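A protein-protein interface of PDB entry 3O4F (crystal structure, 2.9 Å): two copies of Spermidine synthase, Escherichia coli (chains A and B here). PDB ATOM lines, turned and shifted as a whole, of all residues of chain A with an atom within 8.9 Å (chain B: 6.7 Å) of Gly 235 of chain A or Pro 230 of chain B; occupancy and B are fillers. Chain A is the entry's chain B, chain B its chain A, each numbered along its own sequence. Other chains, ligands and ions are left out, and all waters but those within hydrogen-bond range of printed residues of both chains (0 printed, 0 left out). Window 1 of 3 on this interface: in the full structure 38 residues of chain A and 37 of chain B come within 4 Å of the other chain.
Among the printed residues, pairs that only touch across the chains: Phe 21 of chain A with Phe 49 of chain B (3.99 Å), Gly 22 of chain A with Gln 23 of chain B (3.3 Å), Phe 202 of chain A with Phe 49 of chain B (3.8 Å), Phe 202 of chain A with Asp 65 of chain B (3.7 Å), Phe 202 of chain A with Pro 230 of chain B (3.9 Å), Ala 228 of chain A with Ala 228 of chain B (3.7 Å), Pro 230 of chain A with Tyr 233 of chain B (3.8 Å), Pro 230 of chain A with Gly 234 of chain B (3.7 Å), Pro 230 of chain A with Gly 235 of chain B (3.6 Å), Tyr 233 of chain A with Pro 230 of chain B (3.8 Å), Tyr 233 of chain A with Tyr 233 of chain B (3.5 Å), Gly 234 of chain A with Pro 230 of chain B (3.8 Å) and Gly 235 of chain A with Pro 230 of chain B (3.7 Å).
Gly 235 of chain A touches just one residue of chain B: Pro 230.
Printed residues of chain A within 4 Å of Tyr 233 of chain B: Gln 23, Pro 230 and Tyr 233.
Of the printed residues of chain B, Phe 202 of chain A touches Phe 49, Asp 65 and Pro 230.
Of the printed residues of chain B, Gly 22 of chain A touches Gln 23.
Printed residues of chain A within 4 Å of Phe 49 of chain B: Phe 21 (3.99 Å) and Phe 202 (3.8 Å).
Thr 231 of chain A touches none of the printed residues of chain B.
Leu 203 of chain A touches none of the printed residues of chain B.
Of the 12 printed residues of chain B, 8 touch a printed residue of chain A.
Hydrophobic or aromatic side chains of chain B that line the printed part of chain A: Phe 49, Ala 228, Pro 230 and Tyr 233.
Among the printed residues, no Asp or Glu carboxylate lies within 4 Å of a Lys or Arg side-chain nitrogen of the other chain.
Gln 23 of chain A touches Tyr 233 of chain B, and with the chains exchanged Tyr 233 of chain A touches Gln 23 of chain B.
Pro 230 of chain A touches Tyr 233 of chain B, and with the chains exchanged Tyr 233 of chain A touches Pro 230 of chain B.
Pro 230 of chain A touches Gly 234 of chain B, and with the chains exchanged Gly 234 of chain A touches Pro 230 of chain B.
Pro 230 of chain A touches Gly 235 of chain B, and with the chains exchanged Gly 235 of chain A touches Pro 230 of chain B.
The side-chain amide nitrogen (NE2) of Gln 23 of chain A lies within hydrogen-bond range of the backbone carbonyl oxygen (O) of Thr 231 of chain A (2.8 Å).
The side-chain amide nitrogen of Gln 23 of chain B sits at hydrogen-bond distance from the backbone carbonyl oxygen of Thr 231 of chain B (2.7 Å).
OG1 of Thr 231 of chain B sits at hydrogen-bond distance from OD1 of Asp 65 of chain B.
OE1 of Gln 23 of chain B is in hydrogen-bond range of OH of Tyr 233 of chain A, 2.5 Å away.
OH of Tyr 233 of chain B lies close to OE1 of Gln 23 of chain A (2.4 Å).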
ATOM      1  N   PHE A  21       7.018  -8.962 -27.225  1.00  0.00           N
ATOM      2  CA  PHE A  21       7.183  -8.202 -26.004  1.00  0.00           C
ATOM      3  C   PHE A  21       5.871  -8.258 -25.201  1.00  0.00           C
ATOM      4  O   PHE A  21       4.790  -8.548 -25.741  1.00  0.00           O
ATOM      5  CB  PHE A  21       7.475  -6.753 -26.375  1.00  0.00           C
ATOM      6  CG  PHE A  21       6.362  -6.124 -27.143  1.00  0.00           C
ATOM      7  CD1 PHE A  21       6.263  -6.303 -28.513  1.00  0.00           C
ATOM      8  CD2 PHE A  21       5.357  -5.436 -26.490  1.00  0.00           C
ATOM      9  CE1 PHE A  21       5.196  -5.761 -29.223  1.00  0.00           C
ATOM     10  CE2 PHE A  21       4.290  -4.911 -27.191  1.00  0.00           C
ATOM     11  CZ  PHE A  21       4.209  -5.064 -28.550  1.00  0.00           C
ATOM     12  N   GLY A  22       5.946  -7.943 -23.923  1.00  0.00           N
ATOM     13  CA  GLY A  22       4.733  -7.844 -23.152  1.00  0.00           C
ATOM     14  C   GLY A  22       4.895  -7.133 -21.828  1.00  0.00           C
ATOM     15  O   GLY A  22       5.949  -6.559 -21.539  1.00  0.00           O
ATOM     16  N   GLN A  23       3.815  -7.169 -21.041  1.00  0.00           N
ATOM     17  CA  GLN A  23       3.865  -6.796 -19.633  1.00  0.00           C
ATOM     18  C   GLN A  23       3.747  -8.080 -18.809  1.00  0.00           C
ATOM     19  O   GLN A  23       3.142  -9.040 -19.265  1.00  0.00           O
ATOM     20  CB  GLN A  23       2.758  -5.783 -19.295  1.00  0.00           C
ATOM     21  CG  GLN A  23       1.353  -6.325 -19.427  1.00  0.00           C
ATOM     22  CD  GLN A  23       0.273  -5.236 -19.501  1.00  0.00           C
ATOM     23  OE1 GLN A  23       0.225  -4.331 -18.666  1.00  0.00           O
ATOM     24  NE2 GLN A  23      -0.631  -5.363 -20.492  1.00  0.00           N
ATOM     25  N   GLY A 199      -8.129   0.194 -29.626  1.00  0.00           N
ATOM     26  CA  GLY A 199      -6.787  -0.395 -29.482  1.00  0.00           C
ATOM     27  C   GLY A 199      -5.672   0.611 -29.329  1.00  0.00           C
ATOM     28  O   GLY A 199      -5.885   1.788 -29.551  1.00  0.00           O
ATOM     29  N   VAL A 200      -4.481   0.140 -28.946  1.00  0.00           N
ATOM     30  CA  VAL A 200      -3.354   1.056 -28.672  1.00  0.00           C
ATOM     31  C   VAL A 200      -2.737   1.412 -30.004  1.00  0.00           C
ATOM     32  O   VAL A 200      -2.677   0.598 -30.892  1.00  0.00           O
ATOM     33  CB  VAL A 200      -2.297   0.528 -27.644  1.00  0.00           C
ATOM     34  CG1 VAL A 200      -2.884  -0.572 -26.764  1.00  0.00           C
ATOM     35  CG2 VAL A 200      -1.085   0.080 -28.294  1.00  0.00           C
ATOM     36  N   CYS A 201      -2.326   2.657 -30.162  1.00  0.00           N
ATOM     37  CA  CYS A 201      -2.068   3.181 -31.490  1.00  0.00           C
ATOM     38  C   CYS A 201      -0.597   3.233 -31.878  1.00  0.00           C
ATOM     39  O   CYS A 201      -0.263   3.405 -33.049  1.00  0.00           O
ATOM     40  CB  CYS A 201      -2.838   4.509 -31.722  1.00  0.00           C
ATOM     41  SG  CYS A 201      -4.368   4.092 -32.684  1.00  0.00           S
ATOM     42  N   PHE A 202       0.294   2.951 -30.942  1.00  0.00           N
ATOM     43  CA  PHE A 202       1.720   3.060 -31.243  1.00  0.00           C
ATOM     44  C   PHE A 202       2.201   2.113 -32.283  1.00  0.00           C
ATOM     45  O   PHE A 202       2.851   2.560 -33.209  1.00  0.00           O
ATOM     46  CB  PHE A 202       2.598   2.865 -30.018  1.00  0.00           C
ATOM     47  CG  PHE A 202       4.045   3.023 -30.316  1.00  0.00           C
ATOM     48  CD1 PHE A 202       4.558   4.256 -30.685  1.00  0.00           C
ATOM     49  CD2 PHE A 202       4.895   1.959 -30.286  1.00  0.00           C
ATOM     50  CE1 PHE A 202       5.892   4.424 -31.014  1.00  0.00           C
ATOM     51  CE2 PHE A 202       6.263   2.139 -30.610  1.00  0.00           C
ATOM     52  CZ  PHE A 202       6.744   3.377 -30.967  1.00  0.00           C
ATOM     53  N   LEU A 203       1.968   0.823 -32.091  1.00  0.00           N
ATOM     54  CA  LEU A 203       2.452  -0.225 -32.986  1.00  0.00           C
ATOM     55  C   LEU A 203       1.901  -0.231 -34.392  1.00  0.00           C
ATOM     56  O   LEU A 203       2.617  -0.415 -35.356  1.00  0.00           O
ATOM     57  CB  LEU A 203       2.128  -1.568 -32.382  1.00  0.00           C
ATOM     58  CG  LEU A 203       2.830  -1.931 -31.097  1.00  0.00           C
ATOM     59  CD1 LEU A 203       4.292  -1.683 -31.246  1.00  0.00           C
ATOM     60  CD2 LEU A 203       2.246  -1.161 -29.946  1.00  0.00           C
ATOM     61  N   GLN A 226      -8.329   9.989 -27.158  1.00  0.00           N
ATOM     62  CA  GLN A 226      -7.355   9.072 -26.578  1.00  0.00           C
ATOM     63  C   GLN A 226      -7.075   9.237 -25.117  1.00  0.00           C
ATOM     64  O   GLN A 226      -7.275  10.277 -24.540  1.00  0.00           O
ATOM     65  CB  GLN A 226      -6.031   9.129 -27.328  1.00  0.00           C
ATOM     66  CG  GLN A 226      -5.443  10.482 -27.437  1.00  0.00           C
ATOM     67  CD  GLN A 226      -4.704  10.948 -26.194  1.00  0.00           C
ATOM     68  OE1 GLN A 226      -4.382  10.145 -25.286  1.00  0.00           O
ATOM     69  NE2 GLN A 226      -4.415  12.285 -26.148  1.00  0.00           N
ATOM     70  N   ALA A 227      -6.581   8.161 -24.538  1.00  0.00           N
ATOM     71  CA  ALA A 227      -6.246   8.093 -23.138  1.00  0.00           C
ATOM     72  C   ALA A 227      -5.188   7.011 -23.001  1.00  0.00           C
ATOM     73  O   ALA A 227      -5.132   6.108 -23.836  1.00  0.00           O
ATOM     74  CB  ALA A 227      -7.473   7.745 -22.318  1.00  0.00           C
ATOM     75  N   ALA A 228      -4.330   7.116 -21.986  1.00  0.00           N
ATOM     76  CA  ALA A 228      -3.280   6.138 -21.802  1.00  0.00           C
ATOM     77  C   ALA A 228      -3.581   5.299 -20.565  1.00  0.00           C
ATOM     78  O   ALA A 228      -3.494   5.796 -19.441  1.00  0.00           O
ATOM     79  CB  ALA A 228      -1.925   6.826 -21.686  1.00  0.00           C
ATOM     80  N   ILE A 229      -3.933   4.043 -20.781  1.00  0.00           N
ATOM     81  CA  ILE A 229      -4.262   3.142 -19.700  1.00  0.00           C
ATOM     82  C   ILE A 229      -3.083   2.205 -19.425  1.00  0.00           C
ATOM     83  O   ILE A 229      -2.723   1.375 -20.287  1.00  0.00           O
ATOM     84  CB  ILE A 229      -5.493   2.266 -20.066  1.00  0.00           C
ATOM     85  CG1 ILE A 229      -6.743   3.147 -20.213  1.00  0.00           C
ATOM     86  CG2 ILE A 229      -5.656   1.111 -19.055  1.00  0.00           C
ATOM     87  CD1 ILE A 229      -6.823   3.822 -21.571  1.00  0.00           C
ATOM     88  N   PRO A 230      -2.500   2.307 -18.225  1.00  0.00           N
ATOM     89  CA  PRO A 230      -1.223   1.676 -17.889  1.00  0.00           C
ATOM     90  C   PRO A 230      -1.139   0.258 -18.293  1.00  0.00           C
ATOM     91  O   PRO A 230      -0.107  -0.204 -18.722  1.00  0.00           O
ATOM     92  CB  PRO A 230      -1.191   1.735 -16.365  1.00  0.00           C
ATOM     93  CG  PRO A 230      -1.920   2.955 -16.035  1.00  0.00           C
ATOM     94  CD  PRO A 230      -3.057   3.027 -17.072  1.00  0.00           C
ATOM     95  N   THR A 231      -2.241  -0.430 -18.152  1.00  0.00           N
ATOM     96  CA  THR A 231      -2.283  -1.873 -18.251  1.00  0.00           C
ATOM     97  C   THR A 231      -2.627  -2.376 -19.639  1.00  0.00           C
ATOM     98  O   THR A 231      -2.641  -3.573 -19.839  1.00  0.00           O
ATOM     99  CB  THR A 231      -3.299  -2.386 -17.212  1.00  0.00           C
ATOM    100  OG1 THR A 231      -2.819  -1.981 -15.919  1.00  0.00           O
ATOM    101  CG2 THR A 231      -3.637  -3.916 -17.377  1.00  0.00           C
ATOM    102  N   TYR A 232      -2.990  -1.462 -20.544  1.00  0.00           N
ATOM    103  CA  TYR A 232      -3.001  -1.727 -21.980  1.00  0.00           C
ATOM    104  C   TYR A 232      -1.712  -1.144 -22.541  1.00  0.00           C
ATOM    105  O   TYR A 232      -1.596   0.065 -22.797  1.00  0.00           O
ATOM    106  CB  TYR A 232      -4.223  -1.131 -22.690  1.00  0.00           C
ATOM    107  CG  TYR A 232      -5.539  -1.636 -22.188  1.00  0.00           C
ATOM    108  CD1 TYR A 232      -5.707  -2.950 -21.802  1.00  0.00           C
ATOM    109  CD2 TYR A 232      -6.618  -0.797 -22.104  1.00  0.00           C
ATOM    110  CE1 TYR A 232      -6.947  -3.410 -21.334  1.00  0.00           C
ATOM    111  CE2 TYR A 232      -7.847  -1.241 -21.656  1.00  0.00           C
ATOM    112  CZ  TYR A 232      -8.011  -2.548 -21.281  1.00  0.00           C
ATOM    113  OH  TYR A 232      -9.232  -2.977 -20.843  1.00  0.00           O
ATOM    114  N   TYR A 233      -0.755  -2.047 -22.718  1.00  0.00           N
ATOM    115  CA  TYR A 233       0.635  -1.700 -22.914  1.00  0.00           C
ATOM    116  C   TYR A 233       0.802  -0.981 -24.238  1.00  0.00           C
ATOM    117  O   TYR A 233       0.088  -1.275 -25.192  1.00  0.00           O
ATOM    118  CB  TYR A 233       1.476  -2.972 -22.890  1.00  0.00           C
ATOM    119  CG  TYR A 233       2.953  -2.746 -23.006  1.00  0.00           C
ATOM    120  CD1 TYR A 233       3.669  -2.275 -21.936  1.00  0.00           C
ATOM    121  CD2 TYR A 233       3.631  -3.004 -24.187  1.00  0.00           C
ATOM    122  CE1 TYR A 233       5.026  -2.051 -22.027  1.00  0.00           C
ATOM    123  CE2 TYR A 233       4.979  -2.778 -24.293  1.00  0.00           C
ATOM    124  CZ  TYR A 233       5.672  -2.311 -23.209  1.00  0.00           C
ATOM    125  OH  TYR A 233       7.026  -2.107 -23.302  1.00  0.00           O
ATOM    126  N   GLY A 234       1.710  -0.005 -24.278  1.00  0.00           N
ATOM    127  CA  GLY A 234       2.127   0.614 -25.547  1.00  0.00           C
ATOM    128  C   GLY A 234       1.704   2.062 -25.762  1.00  0.00           C
ATOM    129  O   GLY A 234       1.490   2.532 -26.881  1.00  0.00           O
ATOM    130  N   GLY A 235       1.571   2.801 -24.684  1.00  0.00           N
ATOM    131  CA  GLY A 235       1.163   4.184 -24.820  1.00  0.00           C
ATOM    132  C   GLY A 235      -0.331   4.374 -24.902  1.00  0.00           C
ATOM    133  O   GLY A 235      -1.080   3.669 -24.226  1.00  0.00           O
ATOM    134  N   ILE A 236      -0.753   5.347 -25.715  1.00  0.00           N
ATOM    135  CA  ILE A 236      -2.150   5.802 -25.742  1.00  0.00           C
ATOM    136  C   ILE A 236      -2.994   4.805 -26.496  1.00  0.00           C
ATOM    137  O   ILE A 236      -2.517   4.156 -27.418  1.00  0.00           O
ATOM    138  CB  ILE A 236      -2.366   7.216 -26.401  1.00  0.00           C
ATOM    139  CG1 ILE A 236      -2.208   7.146 -27.937  1.00  0.00           C
ATOM    140  CG2 ILE A 236      -1.452   8.238 -25.807  1.00  0.00           C
ATOM    141  CD1 ILE A 236      -2.315   8.449 -28.612  1.00  0.00           C
ATOM    142  N   MET A 237      -4.254   4.745 -26.093  1.00  0.00           N
ATOM    143  CA  MET A 237      -5.300   3.929 -26.694  1.00  0.00           C
ATOM    144  C   MET A 237      -6.259   4.875 -27.385  1.00  0.00           C
ATOM    145  O   MET A 237      -6.415   6.019 -27.026  1.00  0.00           O
ATOM    146  CB  MET A 237      -6.017   3.114 -25.583  1.00  0.00           C
ATOM    147  CG  MET A 237      -7.454   2.719 -25.831  1.00  0.00           C
ATOM    148  SD  MET A 237      -7.989   1.417 -24.699  1.00  0.00           S
ATOM    149  CE  MET A 237      -7.489  -0.016 -25.683  1.00  0.00           C
ATOM    150  N   THR A 238      -6.952   4.375 -28.369  1.00  0.00           N
ATOM    151  CA  THR A 238      -7.733   5.236 -29.203  1.00  0.00           C
ATOM    152  C   THR A 238      -9.160   4.821 -29.138  1.00  0.00           C
ATOM    153  O   THR A 238      -9.457   3.647 -29.228  1.00  0.00           O
ATOM    154  CB  THR A 238      -7.274   5.067 -30.604  1.00  0.00           C
ATOM    155  OG1 THR A 238      -5.828   5.202 -30.644  1.00  0.00           O
ATOM    156  CG2 THR A 238      -7.964   6.076 -31.507  1.00  0.00           C
ATOM    157  N   PHE A 239     -10.041   5.792 -29.014  1.00  0.00           N
ATOM    158  CA  PHE A 239     -11.452   5.534 -28.904  1.00  0.00           C
ATOM    159  C   PHE A 239     -12.142   6.119 -30.140  1.00  0.00           C
ATOM    160  O   PHE A 239     -11.950   7.282 -30.483  1.00  0.00           O
ATOM    161  CB  PHE A 239     -11.950   6.166 -27.636  1.00  0.00           C
ATOM    162  CG  PHE A 239     -11.274   5.651 -26.425  1.00  0.00           C
ATOM    163  CD1 PHE A 239     -11.696   4.496 -25.843  1.00  0.00           C
ATOM    164  CD2 PHE A 239     -10.225   6.324 -25.848  1.00  0.00           C
ATOM    165  CE1 PHE A 239     -11.083   4.005 -24.693  1.00  0.00           C
ATOM    166  CE2 PHE A 239      -9.612   5.856 -24.692  1.00  0.00           C
ATOM    167  CZ  PHE A 239     -10.044   4.699 -24.117  1.00  0.00           C
ATOM    168  N   PRO A 282      -1.566  12.514 -31.593  1.00  0.00           N
ATOM    169  CA  PRO A 282      -0.175  12.627 -31.965  1.00  0.00           C
ATOM    170  C   PRO A 282      -0.020  12.536 -33.446  1.00  0.00           C
ATOM    171  O   PRO A 282      -0.817  11.880 -34.127  1.00  0.00           O
ATOM    172  CB  PRO A 282       0.484  11.425 -31.321  1.00  0.00           C
ATOM    173  CG  PRO A 282      -0.591  10.515 -30.948  1.00  0.00           C
ATOM    174  CD  PRO A 282      -1.869  11.275 -30.881  1.00  0.00           C
ATOM    175  N   TYR A 284       1.841  11.108 -35.735  1.00  0.00           N
ATOM    176  CA  TYR A 284       1.835   9.870 -36.519  1.00  0.00           C
ATOM    177  C   TYR A 284       0.434   9.341 -36.790  1.00  0.00           C
ATOM    178  O   TYR A 284       0.161   8.899 -37.919  1.00  0.00           O
ATOM    179  CB  TYR A 284       2.701   8.778 -35.892  1.00  0.00           C
ATOM    180  CG  TYR A 284       2.178   8.152 -34.656  1.00  0.00           C
ATOM    181  CD1 TYR A 284       2.564   8.616 -33.422  1.00  0.00           C
ATOM    182  CD2 TYR A 284       1.308   7.097 -34.708  1.00  0.00           C
ATOM    183  CE1 TYR A 284       2.092   8.037 -32.233  1.00  0.00           C
ATOM    184  CE2 TYR A 284       0.805   6.507 -33.520  1.00  0.00           C
ATOM    185  CZ  TYR A 284       1.217   6.982 -32.275  1.00  0.00           C
ATOM    186  OH  TYR A 284       0.792   6.437 -31.067  1.00  0.00           O
ATOM    187  N   GLN B  23       7.856  -4.846 -17.742  1.00  0.00           N
ATOM    188  CA  GLN B  23       7.768  -5.109 -19.172  1.00  0.00           C
ATOM    189  C   GLN B  23       8.905  -6.032 -19.543  1.00  0.00           C
ATOM    190  O   GLN B  23       9.961  -5.987 -18.921  1.00  0.00           O
ATOM    191  CB  GLN B  23       7.855  -3.802 -20.002  1.00  0.00           C
ATOM    192  CG  GLN B  23       9.166  -3.041 -19.912  1.00  0.00           C
ATOM    193  CD  GLN B  23       9.005  -1.611 -20.364  1.00  0.00           C
ATOM    194  OE1 GLN B  23       8.324  -1.341 -21.345  1.00  0.00           O
ATOM    195  NE2 GLN B  23       9.617  -0.677 -19.632  1.00  0.00           N
ATOM    196  N   PHE B  49      10.770  -2.771 -30.858  1.00  0.00           N
ATOM    197  CA  PHE B  49      11.283  -1.477 -30.400  1.00  0.00           C
ATOM    198  C   PHE B  49      12.716  -1.186 -30.820  1.00  0.00           C
ATOM    199  O   PHE B  49      13.322  -0.246 -30.318  1.00  0.00           O
ATOM    200  CB  PHE B  49      11.181  -1.389 -28.888  1.00  0.00           C
ATOM    201  CG  PHE B  49       9.784  -1.357 -28.397  1.00  0.00           C
ATOM    202  CD1 PHE B  49       9.042  -0.188 -28.445  1.00  0.00           C
ATOM    203  CD2 PHE B  49       9.201  -2.488 -27.877  1.00  0.00           C
ATOM    204  CE1 PHE B  49       7.752  -0.152 -27.989  1.00  0.00           C
ATOM    205  CE2 PHE B  49       7.901  -2.449 -27.413  1.00  0.00           C
ATOM    206  CZ  PHE B  49       7.188  -1.279 -27.487  1.00  0.00           C
ATOM    207  N   ASP B  65      10.868   4.346 -29.977  1.00  0.00           N
ATOM    208  CA  ASP B  65       9.915   5.252 -29.302  1.00  0.00           C
ATOM    209  C   ASP B  65      10.547   6.470 -28.617  1.00  0.00           C
ATOM    210  O   ASP B  65       9.844   7.308 -28.094  1.00  0.00           O
ATOM    211  CB  ASP B  65       9.060   4.459 -28.318  1.00  0.00           C
ATOM    212  CG  ASP B  65       9.765   4.178 -27.005  1.00  0.00           C
ATOM    213  OD1 ASP B  65       9.017   3.780 -26.088  1.00  0.00           O
ATOM    214  OD2 ASP B  65      11.029   4.316 -26.886  1.00  0.00           O
ATOM    215  N   ILE B  68       9.125  10.205 -28.933  1.00  0.00           N
ATOM    216  CA  ILE B  68       8.012  10.775 -28.205  1.00  0.00           C
ATOM    217  C   ILE B  68       8.605  11.491 -27.053  1.00  0.00           C
ATOM    218  O   ILE B  68       8.279  12.663 -26.835  1.00  0.00           O
ATOM    219  CB  ILE B  68       7.038   9.726 -27.696  1.00  0.00           C
ATOM    220  CG1 ILE B  68       6.381   8.992 -28.874  1.00  0.00           C
ATOM    221  CG2 ILE B  68       5.951  10.350 -26.851  1.00  0.00           C
ATOM    222  CD1 ILE B  68       5.810   7.610 -28.495  1.00  0.00           C
ATOM    223  N   ALA B 228       2.705  10.015 -22.874  1.00  0.00           N
ATOM    224  CA  ALA B 228       2.751   8.604 -22.567  1.00  0.00           C
ATOM    225  C   ALA B 228       3.748   7.907 -23.492  1.00  0.00           C
ATOM    226  O   ALA B 228       3.459   7.728 -24.708  1.00  0.00           O
ATOM    227  CB  ALA B 228       1.386   8.005 -22.739  1.00  0.00           C
ATOM    228  N   ILE B 229       4.890   7.504 -22.908  1.00  0.00           N
ATOM    229  CA  ILE B 229       5.967   6.842 -23.631  1.00  0.00           C
ATOM    230  C   ILE B 229       5.914   5.339 -23.444  1.00  0.00           C
ATOM    231  O   ILE B 229       6.138   4.851 -22.346  1.00  0.00           O
ATOM    232  CB  ILE B 229       7.331   7.337 -23.144  1.00  0.00           C
ATOM    233  CG1 ILE B 229       7.506   8.816 -23.508  1.00  0.00           C
ATOM    234  CG2 ILE B 229       8.498   6.486 -23.733  1.00  0.00           C
ATOM    235  CD1 ILE B 229       6.908   9.738 -22.511  1.00  0.00           C
ATOM    236  N   PRO B 230       5.640   4.592 -24.525  1.00  0.00           N
ATOM    237  CA  PRO B 230       5.282   3.165 -24.422  1.00  0.00           C
ATOM    238  C   PRO B 230       6.192   2.394 -23.499  1.00  0.00           C
ATOM    239  O   PRO B 230       5.760   1.570 -22.704  1.00  0.00           O
ATOM    240  CB  PRO B 230       5.465   2.662 -25.851  1.00  0.00           C
ATOM    241  CG  PRO B 230       5.137   3.829 -26.672  1.00  0.00           C
ATOM    242  CD  PRO B 230       5.664   5.036 -25.924  1.00  0.00           C
ATOM    243  N   THR B 231       7.456   2.717 -23.610  1.00  0.00           N
ATOM    244  CA  THR B 231       8.532   1.927 -23.023  1.00  0.00           C
ATOM    245  C   THR B 231       8.915   2.345 -21.583  1.00  0.00           C
ATOM    246  O   THR B 231       9.732   1.672 -20.932  1.00  0.00           O
ATOM    247  CB  THR B 231       9.724   1.980 -23.961  1.00  0.00           C
ATOM    248  OG1 THR B 231       9.311   1.411 -25.202  1.00  0.00           O
ATOM    249  CG2 THR B 231      10.963   1.311 -23.351  1.00  0.00           C
ATOM    250  N   TYR B 232       8.329   3.454 -21.113  1.00  0.00           N
ATOM    251  CA  TYR B 232       8.285   3.753 -19.685  1.00  0.00           C
ATOM    252  C   TYR B 232       6.921   3.332 -19.141  1.00  0.00           C
ATOM    253  O   TYR B 232       5.926   4.080 -19.237  1.00  0.00           O
ATOM    254  CB  TYR B 232       8.538   5.231 -19.399  1.00  0.00           C
ATOM    255  CG  TYR B 232       9.855   5.732 -19.877  1.00  0.00           C
ATOM    256  CD1 TYR B 232      10.998   4.939 -19.789  1.00  0.00           C
ATOM    257  CD2 TYR B 232       9.975   7.011 -20.409  1.00  0.00           C
ATOM    258  CE1 TYR B 232      12.249   5.419 -20.229  1.00  0.00           C
ATOM    259  CE2 TYR B 232      11.207   7.501 -20.862  1.00  0.00           C
ATOM    260  CZ  TYR B 232      12.335   6.694 -20.766  1.00  0.00           C
ATOM    261  OH  TYR B 232      13.540   7.130 -21.206  1.00  0.00           O
ATOM    262  N   TYR B 233       6.919   2.143 -18.548  1.00  0.00           N
ATOM    263  CA  TYR B 233       5.703   1.410 -18.286  1.00  0.00           C
ATOM    264  C   TYR B 233       4.844   2.114 -17.275  1.00  0.00           C
ATOM    265  O   TYR B 233       5.386   2.697 -16.328  1.00  0.00           O
ATOM    266  CB  TYR B 233       6.052   0.017 -17.768  1.00  0.00           C
ATOM    267  CG  TYR B 233       4.854  -0.859 -17.545  1.00  0.00           C
ATOM    268  CD1 TYR B 233       4.204  -1.441 -18.601  1.00  0.00           C
ATOM    269  CD2 TYR B 233       4.351  -1.077 -16.286  1.00  0.00           C
ATOM    270  CE1 TYR B 233       3.067  -2.226 -18.410  1.00  0.00           C
ATOM    271  CE2 TYR B 233       3.234  -1.880 -16.091  1.00  0.00           C
ATOM    272  CZ  TYR B 233       2.618  -2.442 -17.165  1.00  0.00           C
ATOM    273  OH  TYR B 233       1.538  -3.228 -17.010  1.00  0.00           O
ATOM    274  N   GLY B 234       3.520   2.087 -17.480  1.00  0.00           N
ATOM    275  CA  GLY B 234       2.585   2.593 -16.462  1.00  0.00           C
ATOM    276  C   GLY B 234       1.828   3.865 -16.796  1.00  0.00           C
ATOM    277  O   GLY B 234       1.515   4.669 -15.916  1.00  0.00           O
ATOM    278  N   GLY B 235       1.507   4.042 -18.068  1.00  0.00           N
ATOM    279  CA  GLY B 235       0.716   5.200 -18.470  1.00  0.00           C
ATOM    280  C   GLY B 235       1.566   6.441 -18.633  1.00  0.00           C
ATOM    281  O   GLY B 235       2.712   6.336 -19.120  1.00  0.00           O
